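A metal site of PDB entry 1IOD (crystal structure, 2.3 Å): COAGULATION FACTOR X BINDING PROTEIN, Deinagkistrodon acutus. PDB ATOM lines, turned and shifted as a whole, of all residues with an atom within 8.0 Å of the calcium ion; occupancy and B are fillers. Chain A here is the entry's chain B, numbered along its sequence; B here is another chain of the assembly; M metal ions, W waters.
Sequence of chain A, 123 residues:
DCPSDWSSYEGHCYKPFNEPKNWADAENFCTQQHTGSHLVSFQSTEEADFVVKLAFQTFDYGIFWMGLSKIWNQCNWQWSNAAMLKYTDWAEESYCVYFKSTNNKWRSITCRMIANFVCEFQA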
ATOM      1  N   TYR A   9      25.066 -19.740   0.253  1.00  0.00           N
ATOM      2  CA  TYR A   9      25.451 -18.530  -0.448  1.00  0.00           C
ATOM      3  C   TYR A   9      24.324 -17.514  -0.388  1.00  0.00           C
ATOM      4  O   TYR A   9      23.169 -17.817  -0.727  1.00  0.00           O
ATOM      5  CB  TYR A   9      25.825 -18.819  -1.903  1.00  0.00           C
ATOM      6  CG  TYR A   9      26.024 -17.575  -2.760  1.00  0.00           C
ATOM      7  CD1 TYR A   9      27.273 -16.948  -2.843  1.00  0.00           C
ATOM      8  CD2 TYR A   9      24.964 -17.027  -3.476  1.00  0.00           C
ATOM      9  CE1 TYR A   9      27.457 -15.805  -3.608  1.00  0.00           C
ATOM     10  CE2 TYR A   9      25.125 -15.890  -4.248  1.00  0.00           C
ATOM     11  CZ  TYR A   9      26.371 -15.286  -4.312  1.00  0.00           C
ATOM     12  OH  TYR A   9      26.511 -14.121  -5.017  1.00  0.00           O
ATOM     13  N   HIS A  12      20.971 -18.716   0.690  1.00  0.00           N
ATOM     14  CA  HIS A  12      20.298 -19.822   0.006  1.00  0.00           C
ATOM     15  C   HIS A  12      21.207 -21.046   0.072  1.00  0.00           C
ATOM     16  O   HIS A  12      22.431 -20.910   0.135  1.00  0.00           O
ATOM     17  CB  HIS A  12      19.969 -19.447  -1.451  1.00  0.00           C
ATOM     18  CG  HIS A  12      18.940 -18.363  -1.594  1.00  0.00           C
ATOM     19  ND1 HIS A  12      19.103 -17.116  -1.042  1.00  0.00           N
ATOM     20  CD2 HIS A  12      17.732 -18.349  -2.213  1.00  0.00           C
ATOM     21  CE1 HIS A  12      18.033 -16.371  -1.316  1.00  0.00           C
ATOM     22  NE2 HIS A  12      17.195 -17.096  -2.035  1.00  0.00           N
ATOM     23  N   TYR A  14      22.422 -24.740  -1.610  1.00  0.00           N
ATOM     24  CA  TYR A  14      22.556 -25.442  -2.885  1.00  0.00           C
ATOM     25  C   TYR A  14      23.197 -26.817  -2.688  1.00  0.00           C
ATOM     26  O   TYR A  14      24.078 -26.974  -1.839  1.00  0.00           O
ATOM     27  CB  TYR A  14      23.451 -24.638  -3.840  1.00  0.00           C
ATOM     28  CG  TYR A  14      23.039 -23.191  -3.988  1.00  0.00           C
ATOM     29  CD1 TYR A  14      23.478 -22.225  -3.084  1.00  0.00           C
ATOM     30  CD2 TYR A  14      22.175 -22.786  -5.002  1.00  0.00           C
ATOM     31  CE1 TYR A  14      23.062 -20.894  -3.179  1.00  0.00           C
ATOM     32  CE2 TYR A  14      21.750 -21.461  -5.095  1.00  0.00           C
ATOM     33  CZ  TYR A  14      22.205 -20.531  -4.179  1.00  0.00           C
ATOM     34  OH  TYR A  14      21.777 -19.228  -4.253  1.00  0.00           O
ATOM     35  N   LEU A  39      14.831 -26.698  -8.516  1.00  0.00           N
ATOM     36  CA  LEU A  39      16.024 -26.760  -9.328  1.00  0.00           C
ATOM     37  C   LEU A  39      16.564 -25.343  -9.180  1.00  0.00           C
ATOM     38  O   LEU A  39      15.780 -24.389  -9.033  1.00  0.00           O
ATOM     39  CB  LEU A  39      15.624 -27.040 -10.769  1.00  0.00           C
ATOM     40  CG  LEU A  39      16.213 -28.234 -11.505  1.00  0.00           C
ATOM     41  CD1 LEU A  39      16.511 -29.392 -10.587  1.00  0.00           C
ATOM     42  CD2 LEU A  39      15.217 -28.652 -12.575  1.00  0.00           C
ATOM     43  N   VAL A  40      17.875 -25.190  -9.195  1.00  0.00           N
ATOM     44  CA  VAL A  40      18.464 -23.863  -9.041  1.00  0.00           C
ATOM     45  C   VAL A  40      18.020 -22.820 -10.065  1.00  0.00           C
ATOM     46  O   VAL A  40      17.861 -23.115 -11.256  1.00  0.00           O
ATOM     47  CB  VAL A  40      20.001 -23.945  -9.035  1.00  0.00           C
ATOM     48  CG1 VAL A  40      20.520 -24.356 -10.407  1.00  0.00           C
ATOM     49  CG2 VAL A  40      20.579 -22.599  -8.610  1.00  0.00           C
ATOM     50  N   SER A  41      17.786 -21.609  -9.580  1.00  0.00           N
ATOM     51  CA  SER A  41      17.394 -20.468 -10.399  1.00  0.00           C
ATOM     52  C   SER A  41      18.541 -19.469 -10.307  1.00  0.00           C
ATOM     53  O   SER A  41      19.099 -19.252  -9.231  1.00  0.00           O
ATOM     54  CB  SER A  41      16.112 -19.842  -9.855  1.00  0.00           C
ATOM     55  OG  SER A  41      16.239 -19.553  -8.467  1.00  0.00           O
ATOM     56  N   PHE A  42      18.890 -18.843 -11.425  1.00  0.00           N
ATOM     57  CA  PHE A  42      19.984 -17.883 -11.420  1.00  0.00           C
ATOM     58  C   PHE A  42      19.493 -16.455 -11.469  1.00  0.00           C
ATOM     59  O   PHE A  42      18.734 -16.086 -12.352  1.00  0.00           O
ATOM     60  CB  PHE A  42      20.932 -18.140 -12.577  1.00  0.00           C
ATOM     61  CG  PHE A  42      21.779 -19.365 -12.399  1.00  0.00           C
ATOM     62  CD1 PHE A  42      22.243 -19.718 -11.133  1.00  0.00           C
ATOM     63  CD2 PHE A  42      22.136 -20.141 -13.487  1.00  0.00           C
ATOM     64  CE1 PHE A  42      23.051 -20.835 -10.968  1.00  0.00           C
ATOM     65  CE2 PHE A  42      22.943 -21.261 -13.332  1.00  0.00           C
ATOM     66  CZ  PHE A  42      23.401 -21.607 -12.068  1.00  0.00           C
ATOM     67  N   GLN A  43      19.917 -15.671 -10.488  1.00  0.00           N
ATOM     68  CA  GLN A  43      19.518 -14.267 -10.419  1.00  0.00           C
ATOM     69  C   GLN A  43      20.684 -13.316 -10.631  1.00  0.00           C
ATOM     70  O   GLN A  43      20.474 -12.132 -10.885  1.00  0.00           O
ATOM     71  CB  GLN A  43      18.814 -13.959  -9.100  1.00  0.00           C
ATOM     72  CG  GLN A  43      17.324 -14.311  -9.083  1.00  0.00           C
ATOM     73  CD  GLN A  43      17.027 -15.815  -9.009  1.00  0.00           C
ATOM     74  OE1 GLN A  43      17.785 -16.596  -8.395  1.00  0.00           O
ATOM     75  NE2 GLN A  43      15.912 -16.223  -9.593  1.00  0.00           N
ATOM     76  N   SER A  44      21.909 -13.833 -10.559  1.00  0.00           N
ATOM     77  CA  SER A  44      23.082 -13.005 -10.771  1.00  0.00           C
ATOM     78  C   SER A  44      24.225 -13.860 -11.253  1.00  0.00           C
ATOM     79  O   SER A  44      24.201 -15.089 -11.121  1.00  0.00           O
ATOM     80  CB  SER A  44      23.492 -12.272  -9.482  1.00  0.00           C
ATOM     81  OG  SER A  44      24.048 -13.159  -8.524  1.00  0.00           O
ATOM     82  N   GLU A  47      26.093 -15.700  -8.380  1.00  0.00           N
ATOM     83  CA  GLU A  47      25.355 -16.841  -7.895  1.00  0.00           C
ATOM     84  C   GLU A  47      25.630 -17.974  -8.890  1.00  0.00           C
ATOM     85  O   GLU A  47      25.939 -19.106  -8.494  1.00  0.00           O
ATOM     86  CB  GLU A  47      23.851 -16.575  -7.841  1.00  0.00           C
ATOM     87  CG  GLU A  47      23.091 -17.772  -7.312  1.00  0.00           C
ATOM     88  CD  GLU A  47      21.601 -17.652  -7.399  1.00  0.00           C
ATOM     89  OE1 GLU A  47      21.085 -16.621  -7.869  1.00  0.00           O
ATOM     90  OE2 GLU A  47      20.927 -18.623  -6.980  1.00  0.00           O
ATOM     91  N   ALA A  48      25.588 -17.627 -10.172  1.00  0.00           N
ATOM     92  CA  ALA A  48      25.830 -18.566 -11.255  1.00  0.00           C
ATOM     93  C   ALA A  48      27.231 -19.157 -11.141  1.00  0.00           C
ATOM     94  O   ALA A  48      27.412 -20.374 -11.193  1.00  0.00           O
ATOM     95  CB  ALA A  48      25.638 -17.875 -12.603  1.00  0.00           C
ATOM     96  N   VAL A  51      27.527 -21.616  -8.202  1.00  0.00           N
ATOM     97  CA  VAL A  51      26.960 -22.931  -8.459  1.00  0.00           C
ATOM     98  C   VAL A  51      27.756 -23.752  -9.475  1.00  0.00           C
ATOM     99  O   VAL A  51      27.869 -24.978  -9.336  1.00  0.00           O
ATOM    100  CB  VAL A  51      25.484 -22.794  -8.884  1.00  0.00           C
ATOM    101  CG1 VAL A  51      24.833 -24.164  -8.975  1.00  0.00           C
ATOM    102  CG2 VAL A  51      24.754 -21.927  -7.879  1.00  0.00           C
ATOM    103  N   GLU A 120      18.026 -25.862  -4.983  1.00  0.00           N
ATOM    104  CA  GLU A 120      18.216 -24.657  -4.205  1.00  0.00           C
ATOM    105  C   GLU A 120      16.973 -24.346  -3.382  1.00  0.00           C
ATOM    106  O   GLU A 120      15.854 -24.680  -3.788  1.00  0.00           O
ATOM    107  CB  GLU A 120      18.519 -23.469  -5.126  1.00  0.00           C
ATOM    108  CG  GLU A 120      18.419 -22.100  -4.444  1.00  0.00           C
ATOM    109  CD  GLU A 120      18.447 -20.915  -5.412  1.00  0.00           C
ATOM    110  OE1 GLU A 120      17.828 -20.987  -6.492  1.00  0.00           O
ATOM    111  OE2 GLU A 120      19.060 -19.888  -5.068  1.00  0.00           O
ATOM    112  N   PHE A 121      17.186 -23.780  -2.196  1.00  0.00           N
ATOM    113  CA  PHE A 121      16.085 -23.364  -1.338  1.00  0.00           C
ATOM    114  C   PHE A 121      16.527 -22.219  -0.444  1.00  0.00           C
ATOM    115  O   PHE A 121      17.721 -21.948  -0.277  1.00  0.00           O
ATOM    116  CB  PHE A 121      15.442 -24.508  -0.530  1.00  0.00           C
ATOM    117  CG  PHE A 121      16.298 -25.094   0.549  1.00  0.00           C
ATOM    118  CD1 PHE A 121      16.582 -24.364   1.712  1.00  0.00           C
ATOM    119  CD2 PHE A 121      16.787 -26.388   0.444  1.00  0.00           C
ATOM    120  CE1 PHE A 121      17.334 -24.916   2.735  1.00  0.00           C
ATOM    121  CE2 PHE A 121      17.536 -26.957   1.463  1.00  0.00           C
ATOM    122  CZ  PHE A 121      17.814 -26.220   2.624  1.00  0.00           C
ATOM    123  N   TRP B  83      10.824 -19.166 -13.713  1.00  0.00           N
ATOM    124  CA  TRP B  83      11.670 -20.207 -13.164  1.00  0.00           C
ATOM    125  C   TRP B  83      10.747 -21.212 -12.475  1.00  0.00           C
ATOM    126  O   TRP B  83       9.621 -20.852 -12.106  1.00  0.00           O
ATOM    127  CB  TRP B  83      12.634 -19.632 -12.136  1.00  0.00           C
ATOM    128  CG  TRP B  83      13.745 -18.845 -12.732  1.00  0.00           C
ATOM    129  CD1 TRP B  83      13.797 -17.492 -12.910  1.00  0.00           C
ATOM    130  CD2 TRP B  83      14.982 -19.368 -13.245  1.00  0.00           C
ATOM    131  NE1 TRP B  83      14.999 -17.134 -13.489  1.00  0.00           N
ATOM    132  CE2 TRP B  83      15.742 -18.268 -13.707  1.00  0.00           C
ATOM    133  CE3 TRP B  83      15.514 -20.657 -13.356  1.00  0.00           C
ATOM    134  CZ2 TRP B  83      17.020 -18.423 -14.259  1.00  0.00           C
ATOM    135  CZ3 TRP B  83      16.778 -20.809 -13.908  1.00  0.00           C
ATOM    136  CH2 TRP B  83      17.513 -19.698 -14.351  1.00  0.00           C
ATOM    137  N   ASP B  85      10.558 -21.987  -9.655  1.00  0.00           N
ATOM    138  CA  ASP B  85      10.208 -21.545  -8.311  1.00  0.00           C
ATOM    139  C   ASP B  85       9.169 -20.426  -8.305  1.00  0.00           C
ATOM    140  O   ASP B  85       8.651 -20.076  -7.242  1.00  0.00           O
ATOM    141  CB  ASP B  85      11.462 -21.117  -7.534  1.00  0.00           C
ATOM    142  CG  ASP B  85      12.212 -19.964  -8.185  1.00  0.00           C
ATOM    143  OD1 ASP B  85      11.622 -19.248  -9.025  1.00  0.00           O
ATOM    144  OD2 ASP B  85      13.403 -19.778  -7.859  1.00  0.00           O
ATOM    145  N   SER B  87       9.690 -17.179  -9.629  1.00  0.00           N
ATOM    146  CA  SER B  87      10.317 -15.919  -9.944  1.00  0.00           C
ATOM    147  C   SER B  87      10.462 -15.739 -11.450  1.00  0.00           C
ATOM    148  O   SER B  87      10.681 -16.707 -12.169  1.00  0.00           O
ATOM    149  CB  SER B  87      11.687 -15.835  -9.279  1.00  0.00           C
ATOM    150  OG  SER B  87      12.439 -16.998  -9.530  1.00  0.00           O
HETATM  151 CA    CA M   1      18.452 -18.245  -6.931  1.00  0.00          CA
HETATM  152  O   HOH W   1      16.253 -18.624  -5.943  1.00  0.00           O
HETATM  153  O   HOH W   2      20.086 -17.140  -5.066  1.00  0.00           O
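Water W2 lies within hydrogen-bond range of the side-chain hydroxyl (OH) of Tyr 14 and the side-chain carboxylate (OE1) of Glu 47.
Of the 17 residues printed, 4 come within 4 Å of the calcium ion. Along chain A the residues within 4 Å of the calcium ion span positions 41 to 120.
The side-chain hydroxyl (OH) of Tyr 14 sits close to the side-chain carboxylate (OE2) of Glu 47 (2.9 Å). The side-chain hydroxyl (OG) of Ser 44 sits at hydrogen-bond distance from the backbone NH (N) of Glu 47. The side-chain carboxylate (OE2) of Glu 120 lies close to the side-chain hydroxyl (OH) of Tyr 14. OG of Ser 41 lies within hydrogen-bond range of OD2 of Asp 85 of chain B (2.9 Å).
OE1 of Gln 43 is bound to the calcium ion, at 2.3 Å. Water W1 binds the calcium ion (2.4 Å). The side-chain carboxylate (OE2) of Glu 47 binds the calcium ion (2.5 Å). The side-chain carboxylate (OE2) of Glu 120 binds the calcium ion. The calcium ion is bound by O of Ser 41 (2.6 Å). Water W2 is bound to the calcium ion (2.7 Å). The calcium ion is bound by OE1 of Glu 120 (2.8 Å). The calcium ion has seven donor atoms within binding distance. Slightly farther from the calcium ion lies OG of Ser 41 (3.0 Å).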
